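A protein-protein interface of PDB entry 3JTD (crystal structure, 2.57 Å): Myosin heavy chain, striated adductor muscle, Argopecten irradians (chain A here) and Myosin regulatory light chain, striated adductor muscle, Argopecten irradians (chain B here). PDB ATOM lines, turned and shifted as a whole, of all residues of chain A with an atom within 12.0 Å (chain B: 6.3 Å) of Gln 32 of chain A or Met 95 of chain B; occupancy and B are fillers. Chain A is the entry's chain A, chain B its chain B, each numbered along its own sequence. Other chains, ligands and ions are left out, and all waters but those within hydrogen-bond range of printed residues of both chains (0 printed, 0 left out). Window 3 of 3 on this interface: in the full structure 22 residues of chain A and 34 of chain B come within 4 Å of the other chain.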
ATOM      1  N   LEU A  21     -16.813  14.628  43.422  1.00  0.00           N
ATOM      2  CA  LEU A  21     -16.951  14.128  42.043  1.00  0.00           C
ATOM      3  C   LEU A  21     -18.090  14.784  41.264  1.00  0.00           C
ATOM      4  O   LEU A  21     -17.902  15.222  40.125  1.00  0.00           O
ATOM      5  CB  LEU A  21     -17.123  12.602  42.061  1.00  0.00           C
ATOM      6  CG  LEU A  21     -15.918  11.876  42.687  1.00  0.00           C
ATOM      7  CD1 LEU A  21     -16.247  10.412  42.967  1.00  0.00           C
ATOM      8  CD2 LEU A  21     -14.694  12.034  41.772  1.00  0.00           C
ATOM      9  N   ILE A  22     -19.269  14.867  41.876  1.00  0.00           N
ATOM     10  CA  ILE A  22     -20.393  15.537  41.212  1.00  0.00           C
ATOM     11  C   ILE A  22     -20.100  17.016  40.828  1.00  0.00           C
ATOM     12  O   ILE A  22     -20.277  17.408  39.667  1.00  0.00           O
ATOM     13  CB  ILE A  22     -21.661  15.517  42.087  1.00  0.00           C
ATOM     14  CG1 ILE A  22     -22.236  14.085  42.184  1.00  0.00           C
ATOM     15  CG2 ILE A  22     -22.678  16.491  41.525  1.00  0.00           C
ATOM     16  CD1 ILE A  22     -22.704  13.482  40.867  1.00  0.00           C
ATOM     17  N   ARG A  23     -19.651  17.829  41.790  1.00  0.00           N
ATOM     18  CA  ARG A  23     -19.358  19.242  41.523  1.00  0.00           C
ATOM     19  C   ARG A  23     -18.291  19.413  40.429  1.00  0.00           C
ATOM     20  O   ARG A  23     -18.335  20.369  39.635  1.00  0.00           O
ATOM     21  CB  ARG A  23     -18.965  19.957  42.829  1.00  0.00           C
ATOM     22  CG  ARG A  23     -20.165  20.148  43.787  1.00  0.00           C
ATOM     23  CD  ARG A  23     -19.828  20.937  45.059  1.00  0.00           C
ATOM     24  NE  ARG A  23     -19.103  20.137  46.042  1.00  0.00           N
ATOM     25  CZ  ARG A  23     -19.655  19.483  47.051  1.00  0.00           C
ATOM     26  NH1 ARG A  23     -18.909  18.768  47.885  1.00  0.00           N
ATOM     27  NH2 ARG A  23     -20.950  19.557  47.250  1.00  0.00           N
ATOM     28  N   LYS A  24     -17.362  18.463  40.367  1.00  0.00           N
ATOM     29  CA  LYS A  24     -16.330  18.476  39.331  1.00  0.00           C
ATOM     30  C   LYS A  24     -16.955  18.363  37.922  1.00  0.00           C
ATOM     31  O   LYS A  24     -16.549  19.062  36.997  1.00  0.00           O
ATOM     32  CB  LYS A  24     -15.364  17.316  39.562  1.00  0.00           C
ATOM     33  CG  LYS A  24     -14.400  17.040  38.430  1.00  0.00           C
ATOM     34  CD  LYS A  24     -13.608  18.282  38.090  1.00  0.00           C
ATOM     35  CE  LYS A  24     -12.544  17.980  37.062  1.00  0.00           C
ATOM     36  NZ  LYS A  24     -11.855  19.229  36.643  1.00  0.00           N
ATOM     37  N   ALA A  25     -17.955  17.489  37.784  1.00  0.00           N
ATOM     38  CA  ALA A  25     -18.657  17.248  36.509  1.00  0.00           C
ATOM     39  C   ALA A  25     -19.671  18.324  36.039  1.00  0.00           C
ATOM     40  O   ALA A  25     -20.002  18.372  34.848  1.00  0.00           O
ATOM     41  CB  ALA A  25     -19.353  15.897  36.582  1.00  0.00           C
ATOM     42  N   TYR A  26     -20.137  19.174  36.965  1.00  0.00           N
ATOM     43  CA  TYR A  26     -21.121  20.238  36.703  1.00  0.00           C
ATOM     44  C   TYR A  26     -20.875  21.227  35.584  1.00  0.00           C
ATOM     45  O   TYR A  26     -21.821  21.690  34.921  1.00  0.00           O
ATOM     46  CB  TYR A  26     -21.352  21.046  37.977  1.00  0.00           C
ATOM     47  CG  TYR A  26     -22.514  22.030  37.926  1.00  0.00           C
ATOM     48  CD1 TYR A  26     -23.840  21.584  37.965  1.00  0.00           C
ATOM     49  CD2 TYR A  26     -22.288  23.413  37.831  1.00  0.00           C
ATOM     50  CE1 TYR A  26     -24.911  22.482  37.911  1.00  0.00           C
ATOM     51  CE2 TYR A  26     -23.349  24.321  37.774  1.00  0.00           C
ATOM     52  CZ  TYR A  26     -24.657  23.849  37.813  1.00  0.00           C
ATOM     53  OH  TYR A  26     -25.708  24.742  37.734  1.00  0.00           O
ATOM     54  N   LYS A  27     -19.621  21.580  35.366  1.00  0.00           N
ATOM     55  CA  LYS A  27     -19.313  22.583  34.348  1.00  0.00           C
ATOM     56  C   LYS A  27     -19.408  22.016  32.936  1.00  0.00           C
ATOM     57  O   LYS A  27     -19.791  22.716  31.995  1.00  0.00           O
ATOM     58  CB  LYS A  27     -17.919  23.200  34.610  1.00  0.00           C
ATOM     59  CG  LYS A  27     -17.563  24.401  33.722  1.00  0.00           C
ATOM     60  CD  LYS A  27     -16.329  24.132  32.862  1.00  0.00           C
ATOM     61  CE  LYS A  27     -15.988  25.343  31.985  1.00  0.00           C
ATOM     62  NZ  LYS A  27     -14.723  25.197  31.184  1.00  0.00           N
ATOM     63  N   LYS A  28     -19.042  20.748  32.804  1.00  0.00           N
ATOM     64  CA  LYS A  28     -19.101  20.048  31.523  1.00  0.00           C
ATOM     65  C   LYS A  28     -20.593  19.897  31.166  1.00  0.00           C
ATOM     66  O   LYS A  28     -20.981  19.966  29.998  1.00  0.00           O
ATOM     67  CB  LYS A  28     -18.439  18.678  31.662  1.00  0.00           C
ATOM     68  CG  LYS A  28     -18.500  17.789  30.446  1.00  0.00           C
ATOM     69  CD  LYS A  28     -18.497  16.344  30.915  1.00  0.00           C
ATOM     70  CE  LYS A  28     -19.771  16.057  31.737  1.00  0.00           C
ATOM     71  NZ  LYS A  28     -19.609  15.165  32.924  1.00  0.00           N
ATOM     72  N   LEU A  29     -21.421  19.745  32.191  1.00  0.00           N
ATOM     73  CA  LEU A  29     -22.841  19.617  31.983  1.00  0.00           C
ATOM     74  C   LEU A  29     -23.545  20.870  31.423  1.00  0.00           C
ATOM     75  O   LEU A  29     -24.456  20.751  30.601  1.00  0.00           O
ATOM     76  CB  LEU A  29     -23.491  19.182  33.280  1.00  0.00           C
ATOM     77  CG  LEU A  29     -24.300  17.890  33.159  1.00  0.00           C
ATOM     78  CD1 LEU A  29     -23.625  16.910  32.197  1.00  0.00           C
ATOM     79  CD2 LEU A  29     -24.440  17.279  34.535  1.00  0.00           C
ATOM     80  N   GLN A  30     -23.122  22.060  31.842  1.00  0.00           N
ATOM     81  CA  GLN A  30     -23.730  23.309  31.362  1.00  0.00           C
ATOM     82  C   GLN A  30     -23.268  23.601  29.945  1.00  0.00           C
ATOM     83  O   GLN A  30     -23.999  24.195  29.146  1.00  0.00           O
ATOM     84  CB  GLN A  30     -23.332  24.507  32.238  1.00  0.00           C
ATOM     85  CG  GLN A  30     -23.584  24.356  33.724  1.00  0.00           C
ATOM     86  CD  GLN A  30     -22.759  25.357  34.544  1.00  0.00           C
ATOM     87  OE1 GLN A  30     -21.525  25.353  34.490  1.00  0.00           O
ATOM     88  NE2 GLN A  30     -23.441  26.217  35.299  1.00  0.00           N
ATOM     89  N   ASP A  31     -22.036  23.213  29.642  1.00  0.00           N
ATOM     90  CA  ASP A  31     -21.497  23.441  28.308  1.00  0.00           C
ATOM     91  C   ASP A  31     -22.243  22.536  27.339  1.00  0.00           C
ATOM     92  O   ASP A  31     -22.640  22.962  26.248  1.00  0.00           O
ATOM     93  CB  ASP A  31     -19.989  23.116  28.253  1.00  0.00           C
ATOM     94  CG  ASP A  31     -19.133  24.105  29.058  1.00  0.00           C
ATOM     95  OD1 ASP A  31     -19.600  25.242  29.300  1.00  0.00           O
ATOM     96  OD2 ASP A  31     -17.988  23.763  29.438  1.00  0.00           O
ATOM     97  N   GLN A  32     -22.446  21.284  27.764  1.00  0.00           N
ATOM     98  CA  GLN A  32     -23.112  20.295  26.939  1.00  0.00           C
ATOM     99  C   GLN A  32     -24.576  20.657  26.655  1.00  0.00           C
ATOM    100  O   GLN A  32     -25.099  20.375  25.557  1.00  0.00           O
ATOM    101  CB  GLN A  32     -22.967  18.904  27.588  1.00  0.00           C
ATOM    102  CG  GLN A  32     -21.559  18.352  27.420  1.00  0.00           C
ATOM    103  CD  GLN A  32     -21.313  17.032  28.131  1.00  0.00           C
ATOM    104  OE1 GLN A  32     -21.864  16.765  29.196  1.00  0.00           O
ATOM    105  NE2 GLN A  32     -20.453  16.219  27.557  1.00  0.00           N
ATOM    106  N   ARG A  33     -25.220  21.308  27.618  1.00  0.00           N
ATOM    107  CA  ARG A  33     -26.603  21.724  27.445  1.00  0.00           C
ATOM    108  C   ARG A  33     -26.688  22.714  26.283  1.00  0.00           C
ATOM    109  O   ARG A  33     -27.708  22.789  25.601  1.00  0.00           O
ATOM    110  CB  ARG A  33     -27.125  22.375  28.720  1.00  0.00           C
ATOM    111  CG  ARG A  33     -28.545  22.905  28.615  1.00  0.00           C
ATOM    112  CD  ARG A  33     -28.614  24.295  29.209  1.00  0.00           C
ATOM    113  NE  ARG A  33     -29.745  24.467  30.108  1.00  0.00           N
ATOM    114  CZ  ARG A  33     -29.679  25.114  31.268  1.00  0.00           C
ATOM    115  NH1 ARG A  33     -30.759  25.226  32.024  1.00  0.00           N
ATOM    116  NH2 ARG A  33     -28.531  25.636  31.683  1.00  0.00           N
ATOM    117  N   ILE A  34     -25.616  23.473  26.064  1.00  0.00           N
ATOM    118  CA  ILE A  34     -25.570  24.442  24.966  1.00  0.00           C
ATOM    119  C   ILE A  34     -25.281  23.676  23.676  1.00  0.00           C
ATOM    120  O   ILE A  34     -25.796  24.012  22.605  1.00  0.00           O
ATOM    121  CB  ILE A  34     -24.486  25.520  25.223  1.00  0.00           C
ATOM    122  CG1 ILE A  34     -24.966  26.459  26.336  1.00  0.00           C
ATOM    123  CG2 ILE A  34     -24.191  26.309  23.949  1.00  0.00           C
ATOM    124  CD1 ILE A  34     -23.856  27.195  27.046  1.00  0.00           C
ATOM    125  N   GLY A  35     -24.436  22.658  23.786  1.00  0.00           N
ATOM    126  CA  GLY A  35     -24.141  21.805  22.650  1.00  0.00           C
ATOM    127  C   GLY A  35     -25.390  21.206  22.035  1.00  0.00           C
ATOM    128  O   GLY A  35     -25.640  21.359  20.840  1.00  0.00           O
ATOM    129  N   LEU A  36     -26.178  20.520  22.859  1.00  0.00           N
ATOM    130  CA  LEU A  36     -27.342  19.789  22.372  1.00  0.00           C
ATOM    131  C   LEU A  36     -28.356  20.729  21.730  1.00  0.00           C
ATOM    132  O   LEU A  36     -28.889  20.445  20.657  1.00  0.00           O
ATOM    133  CB  LEU A  36     -27.999  19.007  23.512  1.00  0.00           C
ATOM    134  CG  LEU A  36     -29.018  17.942  23.105  1.00  0.00           C
ATOM    135  CD1 LEU A  36     -28.538  17.180  21.880  1.00  0.00           C
ATOM    136  CD2 LEU A  36     -29.293  16.991  24.260  1.00  0.00           C
ATOM    137  N   SER A  37     -28.618  21.851  22.394  1.00  0.00           N
ATOM    138  CA  SER A  37     -29.550  22.852  21.874  1.00  0.00           C
ATOM    139  C   SER A  37     -29.119  23.302  20.504  1.00  0.00           C
ATOM    140  O   SER A  37     -29.942  23.459  19.606  1.00  0.00           O
ATOM    141  CB  SER A  37     -29.656  24.070  22.781  1.00  0.00           C
ATOM    142  OG  SER A  37     -30.120  23.665  24.054  1.00  0.00           O
ATOM    143  N   VAL A  38     -27.830  23.515  20.319  1.00  0.00           N
ATOM    144  CA  VAL A  38     -27.412  23.939  19.004  1.00  0.00           C
ATOM    145  C   VAL A  38     -27.716  22.845  17.987  1.00  0.00           C
ATOM    146  O   VAL A  38     -28.159  23.140  16.880  1.00  0.00           O
ATOM    147  CB  VAL A  38     -25.902  24.271  18.950  1.00  0.00           C
ATOM    148  CG1 VAL A  38     -25.458  24.473  17.523  1.00  0.00           C
ATOM    149  CG2 VAL A  38     -25.624  25.537  19.751  1.00  0.00           C
ATOM    150  N   ILE A  39     -27.488  21.586  18.369  1.00  0.00           N
ATOM    151  CA  ILE A  39     -27.709  20.458  17.456  1.00  0.00           C
ATOM    152  C   ILE A  39     -29.194  20.179  17.064  1.00  0.00           C
ATOM    153  O   ILE A  39     -29.511  20.105  15.887  1.00  0.00           O
ATOM    154  CB  ILE A  39     -27.022  19.162  18.002  1.00  0.00           C
ATOM    155  CG1 ILE A  39     -25.490  19.321  17.966  1.00  0.00           C
ATOM    156  CG2 ILE A  39     -27.384  17.966  17.127  1.00  0.00           C
ATOM    157  CD1 ILE A  39     -24.756  18.367  18.885  1.00  0.00           C
ATOM    158  N   GLN A  40     -30.080  20.069  18.049  1.00  0.00           N
ATOM    159  CA  GLN A  40     -31.496  19.841  17.788  1.00  0.00           C
ATOM    160  C   GLN A  40     -32.112  20.988  16.964  1.00  0.00           C
ATOM    161  O   GLN A  40     -32.864  20.731  16.015  1.00  0.00           O
ATOM    162  CB  GLN A  40     -32.266  19.645  19.106  1.00  0.00           C
ATOM    163  CG  GLN A  40     -31.915  18.335  19.822  1.00  0.00           C
ATOM    164  CD  GLN A  40     -32.470  18.228  21.245  1.00  0.00           C
ATOM    165  OE1 GLN A  40     -32.562  19.224  21.964  1.00  0.00           O
ATOM    166  NE2 GLN A  40     -32.826  17.007  21.663  1.00  0.00           N
ATOM    167  N   ARG A  41     -31.795  22.239  17.300  1.00  0.00           N
ATOM    168  CA  ARG A  41     -32.321  23.393  16.558  1.00  0.00           C
ATOM    169  C   ARG A  41     -31.893  23.444  15.083  1.00  0.00           C
ATOM    170  O   ARG A  41     -32.713  23.717  14.210  1.00  0.00           O
ATOM    171  CB  ARG A  41     -31.933  24.723  17.254  1.00  0.00           C
ATOM    172  CG  ARG A  41     -32.190  26.008  16.411  1.00  0.00           C
ATOM    173  CD  ARG A  41     -32.244  27.324  17.244  1.00  0.00           C
ATOM    174  NE  ARG A  41     -31.069  27.514  18.094  1.00  0.00           N
ATOM    175  CZ  ARG A  41     -29.881  27.943  17.680  1.00  0.00           C
ATOM    176  NH1 ARG A  41     -28.888  28.041  18.547  1.00  0.00           N
ATOM    177  NH2 ARG A  41     -29.697  28.304  16.414  1.00  0.00           N
ATOM    178  N   ASN A  42     -30.626  23.180  14.785  1.00  0.00           N
ATOM    179  CA  ASN A  42     -30.168  23.246  13.396  1.00  0.00           C
ATOM    180  C   ASN A  42     -30.673  22.101  12.495  1.00  0.00           C
ATOM    181  O   ASN A  42     -31.027  22.322  11.334  1.00  0.00           O
ATOM    182  CB  ASN A  42     -28.639  23.365  13.379  1.00  0.00           C
ATOM    183  CG  ASN A  42     -28.160  24.752  13.825  1.00  0.00           C
ATOM    184  OD1 ASN A  42     -28.225  25.717  13.061  1.00  0.00           O
ATOM    185  ND2 ASN A  42     -27.700  24.857  15.072  1.00  0.00           N
ATOM    186  N   ARG B  90     -20.114  21.736  14.210  1.00  0.00           N
ATOM    187  CA  ARG B  90     -19.104  20.706  14.398  1.00  0.00           C
ATOM    188  C   ARG B  90     -18.504  20.666  15.841  1.00  0.00           C
ATOM    189  O   ARG B  90     -18.254  19.586  16.384  1.00  0.00           O
ATOM    190  CB  ARG B  90     -18.011  20.899  13.339  1.00  0.00           C
ATOM    191  CG  ARG B  90     -16.728  20.125  13.576  1.00  0.00           C
ATOM    192  CD  ARG B  90     -15.796  20.140  12.343  1.00  0.00           C
ATOM    193  NE  ARG B  90     -15.278  21.459  11.941  1.00  0.00           N
ATOM    194  CZ  ARG B  90     -14.491  22.257  12.681  1.00  0.00           C
ATOM    195  NH1 ARG B  90     -14.092  23.420  12.175  1.00  0.00           N
ATOM    196  NH2 ARG B  90     -14.117  21.923  13.921  1.00  0.00           N
ATOM    197  N   ASN B  91     -18.299  21.815  16.493  1.00  0.00           N
ATOM    198  CA  ASN B  91     -17.739  21.781  17.855  1.00  0.00           C
ATOM    199  C   ASN B  91     -18.789  21.439  18.874  1.00  0.00           C
ATOM    200  O   ASN B  91     -18.473  20.968  19.974  1.00  0.00           O
ATOM    201  CB  ASN B  91     -17.025  23.094  18.204  1.00  0.00           C
ATOM    202  CG  ASN B  91     -15.781  23.305  17.349  1.00  0.00           C
ATOM    203  OD1 ASN B  91     -15.175  22.341  16.871  1.00  0.00           O
ATOM    204  ND2 ASN B  91     -15.394  24.549  17.156  1.00  0.00           N
ATOM    205  N   ALA B  92     -20.047  21.669  18.518  1.00  0.00           N
ATOM    206  CA  ALA B  92     -21.146  21.277  19.403  1.00  0.00           C
ATOM    207  C   ALA B  92     -21.074  19.735  19.551  1.00  0.00           C
ATOM    208  O   ALA B  92     -21.112  19.200  20.664  1.00  0.00           O
ATOM    209  CB  ALA B  92     -22.468  21.678  18.794  1.00  0.00           C
ATOM    210  N   PHE B  93     -20.952  19.041  18.412  1.00  0.00           N
ATOM    211  CA  PHE B  93     -20.838  17.577  18.379  1.00  0.00           C
ATOM    212  C   PHE B  93     -19.579  17.112  19.131  1.00  0.00           C
ATOM    213  O   PHE B  93     -19.626  16.165  19.924  1.00  0.00           O
ATOM    214  CB  PHE B  93     -20.750  17.075  16.926  1.00  0.00           C
ATOM    215  CG  PHE B  93     -22.087  16.888  16.240  1.00  0.00           C
ATOM    216  CD1 PHE B  93     -22.364  17.540  15.038  1.00  0.00           C
ATOM    217  CD2 PHE B  93     -23.039  16.009  16.757  1.00  0.00           C
ATOM    218  CE1 PHE B  93     -23.568  17.320  14.353  1.00  0.00           C
ATOM    219  CE2 PHE B  93     -24.251  15.778  16.081  1.00  0.00           C
ATOM    220  CZ  PHE B  93     -24.517  16.435  14.872  1.00  0.00           C
ATOM    221  N   ALA B  94     -18.463  17.799  18.881  1.00  0.00           N
ATOM    222  CA  ALA B  94     -17.185  17.453  19.516  1.00  0.00           C
ATOM    223  C   ALA B  94     -17.212  17.475  21.052  1.00  0.00           C
ATOM    224  O   ALA B  94     -16.423  16.787  21.703  1.00  0.00           O
ATOM    225  CB  ALA B  94     -16.070  18.353  18.968  1.00  0.00           C
ATOM    226  N   MET B  95     -18.121  18.252  21.628  1.00  0.00           N
ATOM    227  CA  MET B  95     -18.276  18.284  23.072  1.00  0.00           C
ATOM    228  C   MET B  95     -18.633  16.911  23.639  1.00  0.00           C
ATOM    229  O   MET B  95     -18.682  16.721  24.855  1.00  0.00           O
ATOM    230  CB  MET B  95     -19.392  19.242  23.466  1.00  0.00           C
ATOM    231  CG  MET B  95     -18.970  20.665  23.646  1.00  0.00           C
ATOM    232  SD  MET B  95     -20.367  21.635  24.184  1.00  0.00           S
ATOM    233  CE  MET B  95     -20.261  23.035  23.032  1.00  0.00           C
ATOM    234  N   PHE B  96     -18.899  15.947  22.765  1.00  0.00           N
ATOM    235  CA  PHE B  96     -19.292  14.611  23.219  1.00  0.00           C
ATOM    236  C   PHE B  96     -18.322  13.499  22.783  1.00  0.00           C
ATOM    237  O   PHE B  96     -18.524  12.336  23.099  1.00  0.00           O
ATOM    238  CB  PHE B  96     -20.730  14.334  22.741  1.00  0.00           C
ATOM    239  CG  PHE B  96     -21.740  15.341  23.246  1.00  0.00           C
ATOM    240  CD1 PHE B  96     -22.310  15.209  24.519  1.00  0.00           C
ATOM    241  CD2 PHE B  96     -22.138  16.411  22.437  1.00  0.00           C
ATOM    242  CE1 PHE B  96     -23.263  16.109  24.978  1.00  0.00           C
ATOM    243  CE2 PHE B  96     -23.091  17.324  22.885  1.00  0.00           C
ATOM    244  CZ  PHE B  96     -23.661  17.174  24.159  1.00  0.00           C
ATOM    245  N   ASP B  97     -17.267  13.890  22.077  1.00  0.00           N
ATOM    246  CA  ASP B  97     -16.228  12.998  21.586  1.00  0.00           C
ATOM    247  C   ASP B  97     -14.970  13.159  22.476  1.00  0.00           C
ATOM    248  O   ASP B  97     -13.936  13.656  22.030  1.00  0.00           O
ATOM    249  CB  ASP B  97     -15.937  13.375  20.128  1.00  0.00           C
ATOM    250  CG  ASP B  97     -14.811  12.565  19.498  1.00  0.00           C
ATOM    251  OD1 ASP B  97     -14.457  11.478  20.008  1.00  0.00           O
ATOM    252  OD2 ASP B  97     -14.289  13.022  18.455  1.00  0.00           O
ATOM    253  N   GLU B  98     -15.064  12.723  23.732  1.00  0.00           N
ATOM    254  CA  GLU B  98     -13.954  12.840  24.686  1.00  0.00           C
ATOM    255  C   GLU B  98     -12.592  12.319  24.211  1.00  0.00           C
ATOM    256  O   GLU B  98     -11.562  12.934  24.487  1.00  0.00           O
ATOM    257  CB  GLU B  98     -14.320  12.160  26.020  1.00  0.00           C
ATOM    258  N   TYR B 108     -25.021   6.234  20.940  1.00  0.00           N
ATOM    259  CA  TYR B 108     -24.883   7.350  21.857  1.00  0.00           C
ATOM    260  C   TYR B 108     -25.604   8.593  21.329  1.00  0.00           C
ATOM    261  O   TYR B 108     -26.409   9.199  22.028  1.00  0.00           O
ATOM    262  CB  TYR B 108     -23.397   7.624  22.077  1.00  0.00           C
ATOM    263  CG  TYR B 108     -23.082   8.692  23.090  1.00  0.00           C
ATOM    264  CD1 TYR B 108     -23.896   8.901  24.189  1.00  0.00           C
ATOM    265  CD2 TYR B 108     -21.962   9.489  22.944  1.00  0.00           C
ATOM    266  CE1 TYR B 108     -23.602   9.880  25.111  1.00  0.00           C
ATOM    267  CE2 TYR B 108     -21.661  10.466  23.859  1.00  0.00           C
ATOM    268  CZ  TYR B 108     -22.480  10.660  24.941  1.00  0.00           C
ATOM    269  OH  TYR B 108     -22.171  11.639  25.850  1.00  0.00           O
ATOM    270  N   TYR B 141     -19.765  12.818  12.450  1.00  0.00           N
ATOM    271  CA  TYR B 141     -20.327  14.168  12.576  1.00  0.00           C
ATOM    272  C   TYR B 141     -19.666  15.247  11.724  1.00  0.00           C
ATOM    273  O   TYR B 141     -20.273  16.270  11.435  1.00  0.00           O
ATOM    274  CB  TYR B 141     -20.380  14.626  14.045  1.00  0.00           C
ATOM    275  CG  TYR B 141     -19.064  14.678  14.800  1.00  0.00           C
ATOM    276  CD1 TYR B 141     -18.711  13.664  15.689  1.00  0.00           C
ATOM    277  CD2 TYR B 141     -18.203  15.771  14.675  1.00  0.00           C
ATOM    278  CE1 TYR B 141     -17.538  13.736  16.445  1.00  0.00           C
ATOM    279  CE2 TYR B 141     -17.022  15.855  15.427  1.00  0.00           C
ATOM    280  CZ  TYR B 141     -16.699  14.832  16.311  1.00  0.00           C
ATOM    281  OH  TYR B 141     -15.543  14.892  17.048  1.00  0.00           O
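O of Asp 31 of chain A sits close to SD of Met 95 of chain B.
NE2 of Gln 32 of chain A lies within hydrogen-bond range of O of Met 95 of chain B, at 3.3 Å.
O of Lys 28 of chain A sits close to OE1 of Gln 32 of chain A (3.4 Å).
The side-chain carboxylate (OD2) of Asp 31 of chain A is in salt-bridge range of the side-chain amino group (NZ) of Lys 27 of chain A (3.97 Å).
Phe 96 of chain B touches Gln 32 of chain A (CD1 to NE2, 3.7 Å).
O of Gly 35 of chain A touches CB of Ala 92 of chain B, 3.8 Å away.
CG1 of Ile 39 of chain A touches CB of Ala 92 of chain B, 3.9 Å away.
Phe 93 of chain B touches Ile 39 of chain A.
Printed residues of chain B within 4 Å of Asp 31 of chain A: Met 95 (3.3 Å).
Gln 32 of chain A touches two residues of chain B.
Arg 33 of chain A touches none of the printed residues of chain B.
Of the printed residues of chain B, Gly 35 of chain A touches Ala 92 (3.8 Å).
Asn 42 of chain A touches none of the printed residues of chain B.
No residue of chain A comes within 4 Å of Asn 91 of chain B.
Of the printed residues of chain A, Phe 93 of chain B touches Ile 39.
Met 95 of chain B touches just these residues of chain A: Asp 31 (3.3 Å) and Gln 32 (3.3 Å).
No residue of chain A comes within 4 Å of Asp 97 of chain B.
Printed residues of chain B that touch a printed residue of chain A: Ala 92, Phe 93, Met 95 and Phe 96.
Hydrophobic or aromatic side chains of chain B within 4 Å of the printed part of chain A: Ala 92, Phe 93, Met 95 and Phe 96.
Of the 22 printed residues of chain A, 4 touch a printed residue of chain B.
Printed residues of chain A that touch a printed residue of chain B: Asp 31, Gln 32, Gly 35 and Ile 39.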
